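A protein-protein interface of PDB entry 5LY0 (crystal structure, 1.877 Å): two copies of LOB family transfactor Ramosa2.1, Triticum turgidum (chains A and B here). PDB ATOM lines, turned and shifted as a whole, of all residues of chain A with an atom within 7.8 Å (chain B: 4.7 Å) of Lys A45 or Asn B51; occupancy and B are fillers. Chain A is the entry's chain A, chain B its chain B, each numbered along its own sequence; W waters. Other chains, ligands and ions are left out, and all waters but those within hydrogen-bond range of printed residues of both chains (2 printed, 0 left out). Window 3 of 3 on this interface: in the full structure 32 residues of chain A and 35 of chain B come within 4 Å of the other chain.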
ATOM      1  N   PHE A  17      16.949  -1.315  -0.411  1.00  0.00           N
ATOM      2  CA  PHE A  17      15.560  -1.653  -0.709  1.00  0.00           C
ATOM      3  C   PHE A  17      14.836  -0.470  -1.342  1.00  0.00           C
ATOM      4  O   PHE A  17      14.164  -0.613  -2.369  1.00  0.00           O
ATOM      5  CB  PHE A  17      14.850  -2.099   0.570  1.00  0.00           C
ATOM      6  CG  PHE A  17      13.429  -2.546   0.357  1.00  0.00           C
ATOM      7  CD1 PHE A  17      12.407  -1.619   0.223  1.00  0.00           C
ATOM      8  CD2 PHE A  17      13.114  -3.895   0.301  1.00  0.00           C
ATOM      9  CE1 PHE A  17      11.102  -2.027   0.027  1.00  0.00           C
ATOM     10  CE2 PHE A  17      11.809  -4.307   0.107  1.00  0.00           C
ATOM     11  CZ  PHE A  17      10.802  -3.373  -0.029  1.00  0.00           C
ATOM     12  N   GLN A  38      16.227  -9.047   4.549  1.00  0.00           N
ATOM     13  CA  GLN A  38      14.858  -9.463   4.836  1.00  0.00           C
ATOM     14  C   GLN A  38      14.315  -8.766   6.074  1.00  0.00           C
ATOM     15  O   GLN A  38      13.105  -8.533   6.173  1.00  0.00           O
ATOM     16  CB  GLN A  38      14.788 -10.979   5.009  1.00  0.00           C
ATOM     17  CG  GLN A  38      15.039 -11.766   3.731  1.00  0.00           C
ATOM     18  CD  GLN A  38      13.875 -11.696   2.760  1.00  0.00           C
ATOM     19  OE1 GLN A  38      12.804 -11.186   3.089  1.00  0.00           O
ATOM     20  NE2 GLN A  38      14.082 -12.212   1.555  1.00  0.00           N
ATOM     21  N   LYS A  39      15.186  -8.431   7.028  1.00  0.00           N
ATOM     22  CA  LYS A  39      14.735  -7.708   8.212  1.00  0.00           C
ATOM     23  C   LYS A  39      14.058  -6.399   7.825  1.00  0.00           C
ATOM     24  O   LYS A  39      12.968  -6.083   8.316  1.00  0.00           O
ATOM     25  CB  LYS A  39      15.912  -7.448   9.154  1.00  0.00           C
ATOM     26  CG  LYS A  39      15.486  -6.893  10.502  1.00  0.00           C
ATOM     27  CD  LYS A  39      16.631  -6.868  11.502  1.00  0.00           C
ATOM     28  CE  LYS A  39      17.636  -5.780  11.180  1.00  0.00           C
ATOM     29  NZ  LYS A  39      18.553  -5.522  12.327  1.00  0.00           N
ATOM     30  N   PHE A  40      14.687  -5.620   6.943  1.00  0.00           N
ATOM     31  CA  PHE A  40      14.057  -4.373   6.528  1.00  0.00           C
ATOM     32  C   PHE A  40      12.829  -4.634   5.667  1.00  0.00           C
ATOM     33  O   PHE A  40      11.806  -3.955   5.817  1.00  0.00           O
ATOM     34  CB  PHE A  40      15.029  -3.481   5.766  1.00  0.00           C
ATOM     35  CG  PHE A  40      14.412  -2.184   5.358  1.00  0.00           C
ATOM     36  CD1 PHE A  40      14.292  -1.154   6.270  1.00  0.00           C
ATOM     37  CD2 PHE A  40      13.891  -2.015   4.087  1.00  0.00           C
ATOM     38  CE1 PHE A  40      13.696   0.037   5.916  1.00  0.00           C
ATOM     39  CE2 PHE A  40      13.295  -0.825   3.724  1.00  0.00           C
ATOM     40  CZ  PHE A  40      13.196   0.204   4.641  1.00  0.00           C
ATOM     41  N   ALA A  41      12.915  -5.593   4.742  1.00  0.00           N
ATOM     42  CA  ALA A  41      11.771  -5.897   3.887  1.00  0.00           C
ATOM     43  C   ALA A  41      10.528  -6.195   4.718  1.00  0.00           C
ATOM     44  O   ALA A  41       9.431  -5.721   4.401  1.00  0.00           O
ATOM     45  CB  ALA A  41      12.098  -7.078   2.972  1.00  0.00           C
ATOM     46  N   ASN A  42      10.680  -6.973   5.791  1.00  0.00           N
ATOM     47  CA  ASN A  42       9.536  -7.303   6.637  1.00  0.00           C
ATOM     48  C   ASN A  42       9.019  -6.070   7.364  1.00  0.00           C
ATOM     49  O   ASN A  42       7.810  -5.817   7.401  1.00  0.00           O
ATOM     50  CB  ASN A  42       9.918  -8.384   7.648  1.00  0.00           C
ATOM     51  CG  ASN A  42      10.255  -9.706   6.996  1.00  0.00           C
ATOM     52  OD1 ASN A  42       9.908  -9.952   5.840  1.00  0.00           O
ATOM     53  ND2 ASN A  42      10.931 -10.572   7.744  1.00  0.00           N
ATOM     54  N   VAL A  43       9.924  -5.298   7.967  1.00  0.00           N
ATOM     55  CA  VAL A  43       9.510  -4.113   8.711  1.00  0.00           C
ATOM     56  C   VAL A  43       8.839  -3.114   7.777  1.00  0.00           C
ATOM     57  O   VAL A  43       7.852  -2.463   8.140  1.00  0.00           O
ATOM     58  CB  VAL A  43      10.720  -3.500   9.437  1.00  0.00           C
ATOM     59  CG1 VAL A  43      10.359  -2.167  10.059  1.00  0.00           C
ATOM     60  CG2 VAL A  43      11.224  -4.456  10.506  1.00  0.00           C
ATOM     61  N   HIS A  44       9.361  -2.980   6.557  1.00  0.00           N
ATOM     62  CA  HIS A  44       8.755  -2.075   5.586  1.00  0.00           C
ATOM     63  C   HIS A  44       7.346  -2.524   5.220  1.00  0.00           C
ATOM     64  O   HIS A  44       6.427  -1.703   5.130  1.00  0.00           O
ATOM     65  CB  HIS A  44       9.636  -1.993   4.340  1.00  0.00           C
ATOM     66  CG  HIS A  44       9.133  -1.036   3.304  1.00  0.00           C
ATOM     67  ND1 HIS A  44       8.488  -1.448   2.160  1.00  0.00           N
ATOM     68  CD2 HIS A  44       9.185   0.315   3.243  1.00  0.00           C
ATOM     69  CE1 HIS A  44       8.164  -0.391   1.435  1.00  0.00           C
ATOM     70  NE2 HIS A  44       8.575   0.691   2.070  1.00  0.00           N
ATOM     71  N   LYS A  45       7.154  -3.830   5.019  1.00  0.00           N
ATOM     72  CA  LYS A  45       5.842  -4.345   4.637  1.00  0.00           C
ATOM     73  C   LYS A  45       4.810  -4.112   5.733  1.00  0.00           C
ATOM     74  O   LYS A  45       3.665  -3.740   5.450  1.00  0.00           O
ATOM     75  CB  LYS A  45       5.950  -5.838   4.314  1.00  0.00           C
ATOM     76  CG  LYS A  45       4.620  -6.550   4.082  1.00  0.00           C
ATOM     77  CD  LYS A  45       4.854  -8.002   3.681  1.00  0.00           C
ATOM     78  CE  LYS A  45       3.607  -8.644   3.086  1.00  0.00           C
ATOM     79  NZ  LYS A  45       2.533  -8.861   4.094  1.00  0.00           N
ATOM     80  N   VAL A  46       5.190  -4.329   6.987  1.00  0.00           N
ATOM     81  CA  VAL A  46       4.234  -4.309   8.091  1.00  0.00           C
ATOM     82  C   VAL A  46       4.031  -2.897   8.629  1.00  0.00           C
ATOM     83  O   VAL A  46       2.896  -2.440   8.793  1.00  0.00           O
ATOM     84  CB  VAL A  46       4.702  -5.276   9.200  1.00  0.00           C
ATOM     85  CG1 VAL A  46       3.806  -5.175  10.430  1.00  0.00           C
ATOM     86  CG2 VAL A  46       4.725  -6.707   8.674  1.00  0.00           C
ATOM     87  N   PHE A  47       5.119  -2.185   8.919  1.00  0.00           N
ATOM     88  CA  PHE A  47       5.048  -0.873   9.549  1.00  0.00           C
ATOM     89  C   PHE A  47       5.260   0.276   8.573  1.00  0.00           C
ATOM     90  O   PHE A  47       4.641   1.333   8.728  1.00  0.00           O
ATOM     91  CB  PHE A  47       6.084  -0.780  10.674  1.00  0.00           C
ATOM     92  CG  PHE A  47       5.905  -1.819  11.742  1.00  0.00           C
ATOM     93  CD1 PHE A  47       4.919  -1.678  12.705  1.00  0.00           C
ATOM     94  CD2 PHE A  47       6.723  -2.938  11.786  1.00  0.00           C
ATOM     95  CE1 PHE A  47       4.750  -2.632  13.686  1.00  0.00           C
ATOM     96  CE2 PHE A  47       6.557  -3.895  12.766  1.00  0.00           C
ATOM     97  CZ  PHE A  47       5.569  -3.741  13.718  1.00  0.00           C
ATOM     98  N   GLY A  48       6.124   0.101   7.577  1.00  0.00           N
ATOM     99  CA  GLY A  48       6.415   1.162   6.632  1.00  0.00           C
ATOM    100  C   GLY A  48       7.612   1.995   7.049  1.00  0.00           C
ATOM    101  O   GLY A  48       7.814   2.257   8.239  1.00  0.00           O
ATOM    102  N   ALA A  49       8.410   2.426   6.069  1.00  0.00           N
ATOM    103  CA  ALA A  49       9.637   3.154   6.378  1.00  0.00           C
ATOM    104  C   ALA A  49       9.344   4.457   7.113  1.00  0.00           C
ATOM    105  O   ALA A  49      10.074   4.834   8.039  1.00  0.00           O
ATOM    106  CB  ALA A  49      10.414   3.431   5.093  1.00  0.00           C
ATOM    107  N   ASN A  51       6.878   5.247   9.163  1.00  0.00           N
ATOM    108  CA  ASN A  51       6.544   5.017  10.565  1.00  0.00           C
ATOM    109  C   ASN A  51       7.780   4.654  11.377  1.00  0.00           C
ATOM    110  O   ASN A  51       7.914   5.069  12.534  1.00  0.00           O
ATOM    111  CB  ASN A  51       5.488   3.916  10.678  1.00  0.00           C
ATOM    112  CG  ASN A  51       4.076   4.437  10.491  1.00  0.00           C
ATOM    113  OD1 ASN A  51       3.816   5.628  10.652  1.00  0.00           O
ATOM    114  ND2 ASN A  51       3.153   3.542  10.159  1.00  0.00           N
ATOM    115  N   ALA A  75       7.413  -7.938  12.845  1.00  0.00           N
ATOM    116  CA  ALA A  75       7.135  -7.990  11.415  1.00  0.00           C
ATOM    117  C   ALA A  75       7.332  -9.395  10.860  1.00  0.00           C
ATOM    118  O   ALA A  75       6.526  -9.866  10.048  1.00  0.00           O
ATOM    119  CB  ALA A  75       8.024  -6.993  10.674  1.00  0.00           C
ATOM    120  N   ARG A  78       4.408 -11.499  11.621  1.00  0.00           N
ATOM    121  CA  ARG A  78       3.226 -11.214  10.817  1.00  0.00           C
ATOM    122  C   ARG A  78       3.379 -11.723   9.387  1.00  0.00           C
ATOM    123  O   ARG A  78       2.375 -12.015   8.726  1.00  0.00           O
ATOM    124  CB  ARG A  78       2.939  -9.712  10.831  1.00  0.00           C
ATOM    125  CG  ARG A  78       1.596  -9.328  10.229  1.00  0.00           C
ATOM    126  CD  ARG A  78       0.976  -8.127  10.937  1.00  0.00           C
ATOM    127  NE  ARG A  78       0.389  -8.474  12.231  1.00  0.00           N
ATOM    128  CZ  ARG A  78      -0.773  -9.102  12.386  1.00  0.00           C
ATOM    129  NH1 ARG A  78      -1.482  -9.473  11.327  1.00  0.00           N
ATOM    130  NH2 ARG A  78      -1.228  -9.370  13.603  1.00  0.00           N
ATOM    131  N   VAL A  79       4.615 -11.842   8.897  1.00  0.00           N
ATOM    132  CA  VAL A  79       4.851 -12.519   7.627  1.00  0.00           C
ATOM    133  C   VAL A  79       4.546 -14.005   7.759  1.00  0.00           C
ATOM    134  O   VAL A  79       3.956 -14.617   6.860  1.00  0.00           O
ATOM    135  CB  VAL A  79       6.298 -12.274   7.157  1.00  0.00           C
ATOM    136  CG1 VAL A  79       6.705 -13.258   6.054  1.00  0.00           C
ATOM    137  CG2 VAL A  79       6.455 -10.844   6.666  1.00  0.00           C
ATOM    138  N   PRO A  82      -0.024 -14.100   8.945  1.00  0.00           N
ATOM    139  CA  PRO A  82      -0.635 -12.824   8.537  1.00  0.00           C
ATOM    140  C   PRO A  82      -1.885 -12.445   9.317  1.00  0.00           C
ATOM    141  O   PRO A  82      -2.274 -11.271   9.289  1.00  0.00           O
ATOM    142  CB  PRO A  82      -0.957 -13.052   7.053  1.00  0.00           C
ATOM    143  CG  PRO A  82      -0.015 -14.117   6.616  1.00  0.00           C
ATOM    144  CD  PRO A  82       0.154 -15.015   7.803  1.00  0.00           C
ATOM    145  N   PHE B  47       0.704   1.074  12.294  1.00  0.00           N
ATOM    146  CA  PHE B  47       0.785   0.411  11.000  1.00  0.00           C
ATOM    147  C   PHE B  47       0.477   1.335   9.832  1.00  0.00           C
ATOM    148  O   PHE B  47       1.083   1.189   8.765  1.00  0.00           O
ATOM    149  CB  PHE B  47      -0.175  -0.784  10.960  1.00  0.00           C
ATOM    150  CG  PHE B  47       0.114  -1.824  12.004  1.00  0.00           C
ATOM    151  CD1 PHE B  47       1.171  -2.705  11.848  1.00  0.00           C
ATOM    152  CD2 PHE B  47      -0.673  -1.924  13.141  1.00  0.00           C
ATOM    153  CE1 PHE B  47       1.441  -3.662  12.805  1.00  0.00           C
ATOM    154  CE2 PHE B  47      -0.408  -2.880  14.102  1.00  0.00           C
ATOM    155  CZ  PHE B  47       0.650  -3.751  13.933  1.00  0.00           C
ATOM    156  N   GLY B  48      -0.436   2.284  10.007  1.00  0.00           N
ATOM    157  CA  GLY B  48      -0.816   3.176   8.930  1.00  0.00           C
ATOM    158  C   GLY B  48      -2.059   2.693   8.216  1.00  0.00           C
ATOM    159  O   GLY B  48      -2.164   1.511   7.872  1.00  0.00           O
ATOM    160  N   ALA B  49      -3.010   3.602   7.982  1.00  0.00           N
ATOM    161  CA  ALA B  49      -4.276   3.214   7.370  1.00  0.00           C
ATOM    162  C   ALA B  49      -4.055   2.507   6.039  1.00  0.00           C
ATOM    163  O   ALA B  49      -4.763   1.548   5.709  1.00  0.00           O
ATOM    164  CB  ALA B  49      -5.161   4.446   7.177  1.00  0.00           C
ATOM    165  N   SER B  50      -3.070   2.960   5.262  1.00  0.00           N
ATOM    166  CA  SER B  50      -2.847   2.390   3.937  1.00  0.00           C
ATOM    167  C   SER B  50      -2.325   0.962   4.034  1.00  0.00           C
ATOM    168  O   SER B  50      -2.789   0.072   3.309  1.00  0.00           O
ATOM    169  CB  SER B  50      -1.878   3.270   3.147  1.00  0.00           C
ATOM    170  OG  SER B  50      -2.416   4.566   2.954  1.00  0.00           O
ATOM    171  N   ASN B  51      -1.354   0.720   4.920  1.00  0.00           N
ATOM    172  CA  ASN B  51      -0.864  -0.641   5.115  1.00  0.00           C
ATOM    173  C   ASN B  51      -1.987  -1.566   5.565  1.00  0.00           C
ATOM    174  O   ASN B  51      -2.092  -2.702   5.093  1.00  0.00           O
ATOM    175  CB  ASN B  51       0.277  -0.653   6.136  1.00  0.00           C
ATOM    176  CG  ASN B  51       1.651  -0.677   5.486  1.00  0.00           C
ATOM    177  OD1 ASN B  51       1.787  -0.984   4.300  1.00  0.00           O
ATOM    178  ND2 ASN B  51       2.679  -0.364   6.267  1.00  0.00           N
ATOM    179  N   VAL B  52      -2.847  -1.089   6.464  1.00  0.00           N
ATOM    180  CA  VAL B  52      -3.914  -1.933   6.995  1.00  0.00           C
ATOM    181  C   VAL B  52      -4.877  -2.335   5.885  1.00  0.00           C
ATOM    182  O   VAL B  52      -5.262  -3.504   5.767  1.00  0.00           O
ATOM    183  CB  VAL B  52      -4.636  -1.212   8.145  1.00  0.00           C
ATOM    184  CG1 VAL B  52      -5.858  -2.002   8.614  1.00  0.00           C
ATOM    185  CG2 VAL B  52      -3.677  -1.000   9.288  1.00  0.00           C
ATOM    186  N   THR B  53      -5.284  -1.372   5.055  1.00  0.00           N
ATOM    187  CA  THR B  53      -6.117  -1.709   3.905  1.00  0.00           C
ATOM    188  C   THR B  53      -5.414  -2.730   3.022  1.00  0.00           C
ATOM    189  O   THR B  53      -6.025  -3.705   2.569  1.00  0.00           O
ATOM    190  CB  THR B  53      -6.445  -0.451   3.099  1.00  0.00           C
ATOM    191  OG1 THR B  53      -6.933   0.574   3.975  1.00  0.00           O
ATOM    192  CG2 THR B  53      -7.495  -0.754   2.039  1.00  0.00           C
ATOM    193  N   LYS B  54      -4.123  -2.515   2.774  1.00  0.00           N
ATOM    194  CA  LYS B  54      -3.337  -3.437   1.966  1.00  0.00           C
ATOM    195  C   LYS B  54      -3.297  -4.826   2.594  1.00  0.00           C
ATOM    196  O   LYS B  54      -3.533  -5.835   1.919  1.00  0.00           O
ATOM    197  CB  LYS B  54      -1.932  -2.861   1.804  1.00  0.00           C
ATOM    198  CG  LYS B  54      -1.004  -3.607   0.875  1.00  0.00           C
ATOM    199  CD  LYS B  54       0.090  -2.655   0.409  1.00  0.00           C
ATOM    200  CE  LYS B  54       1.410  -3.355   0.142  1.00  0.00           C
ATOM    201  NZ  LYS B  54       1.820  -3.216  -1.280  1.00  0.00           N
ATOM    202  N   LEU B  55      -3.005  -4.897   3.895  1.00  0.00           N
ATOM    203  CA  LEU B  55      -2.870  -6.193   4.553  1.00  0.00           C
ATOM    204  C   LEU B  55      -4.209  -6.911   4.677  1.00  0.00           C
ATOM    205  O   LEU B  55      -4.257  -8.143   4.582  1.00  0.00           O
ATOM    206  CB  LEU B  55      -2.224  -6.013   5.928  1.00  0.00           C
ATOM    207  CG  LEU B  55      -0.689  -6.040   5.951  1.00  0.00           C
ATOM    208  CD1 LEU B  55      -0.078  -5.053   4.960  1.00  0.00           C
ATOM    209  CD2 LEU B  55      -0.166  -5.763   7.354  1.00  0.00           C
ATOM    210  N   GLU B  58      -5.201  -8.648   1.439  1.00  0.00           N
ATOM    211  CA  GLU B  58      -4.444  -9.862   1.159  1.00  0.00           C
ATOM    212  C   GLU B  58      -5.033 -11.095   1.833  1.00  0.00           C
ATOM    213  O   GLU B  58      -4.598 -12.210   1.524  1.00  0.00           O
ATOM    214  CB  GLU B  58      -2.992  -9.683   1.607  1.00  0.00           C
ATOM    215  CG  GLU B  58      -2.190  -8.711   0.751  1.00  0.00           C
ATOM    216  CD  GLU B  58      -0.762  -8.548   1.236  1.00  0.00           C
ATOM    217  OE1 GLU B  58      -0.357  -9.288   2.158  1.00  0.00           O
ATOM    218  OE2 GLU B  58      -0.045  -7.678   0.695  1.00  0.00           O
HETATM  219  O   HOH W   1       4.347  -0.733   3.678  1.00  0.00           O
HETATM  220  O   HOH W   2       2.034  -3.650   3.034  1.00  0.00           O
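Of the 10 printed residues of chain B, 5 touch a printed residue of chain A.
Hydrophobic or aromatic side chains of chain A that line the printed part of chain B: Val A46 and Phe A47.
The side-chain carboxylate of Glu B58 lies within salt-bridge range of the side-chain amino group of Lys A45, at 3.5 Å.
The backbone carbonyl oxygen (O) of Val A46 lies within hydrogen-bond range of the side-chain amide nitrogen (ND2) of Asn B51, at 3.3 Å.
O of Phe B47 is in hydrogen-bond range of ND2 of Asn A51 (3.4 Å).
Gln A38 touches none of the printed residues of chain B.
Of the printed residues of chain B, Lys A45 touches Asn B51 (3.5 Å), Leu B55 (3.997 Å) and Glu B58 (3.5 Å).
Of the printed residues of chain B, Phe A47 touches Phe B47 (3.6 Å) and Asn B51 (3.5 Å).
Printed residues of chain A within 4 Å of Gly B48: Asn A51.
Ala B49 touches none of the printed residues of chain A.
Of chain A, only Lys A45 (3.5 Å), Val A46 (3.3 Å), Phe A47 (3.5 Å) and Gly A48 (3.7 Å) come within 4 Å of Asn B51.
The nearest printed residue of chain B that does not touch Lys A45 is Lys B54 (5.8 Å).
The backbone carbonyl oxygen (O) of Val A43 lies within hydrogen-bond range of the backbone NH (N) of Gly A48, at 3.1 Å.
O of Phe A47 sits at hydrogen-bond distance from ND2 of Asn A51 (3.0 Å).
O of Phe B47 lies close to ND2 of Asn B51 (3.3 Å).
Phe B47 touches its own counterpart, Phe A47.
Phe A47 touches Asn B51, and with the chains exchanged Asn A51 touches Phe B47.
Gly A48 touches Asn B51, and with the chains exchanged Asn A51 touches Gly B48.
4 positions are printed for both chains.
Of the 10 pairs that touch across the chains among the printed residues, 5 have their exchanged pair printed and touching as well.
Water W1 bridges OD1 of Asn B51 (2.6 Å) and O of His A44 (2.7 Å).
Water W2 bridges the backbone carbonyl oxygen of Lys A45 and the side-chain amide oxygen of Asn B51.
OD1 of Asn B51 touches O of Lys A45 (3.5 Å).
Lys A45 touches Leu B55.
Val A46 touches Phe B47 (O to CD1, 3.5 Å).
O of Phe A47 touches O of Phe B47, at 3.6 Å.
Asn B51 touches Phe A47.
Gly A48 touches Asn B51.
ND2 of Asn A51 touches N of Gly B48, at 3.8 Å.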
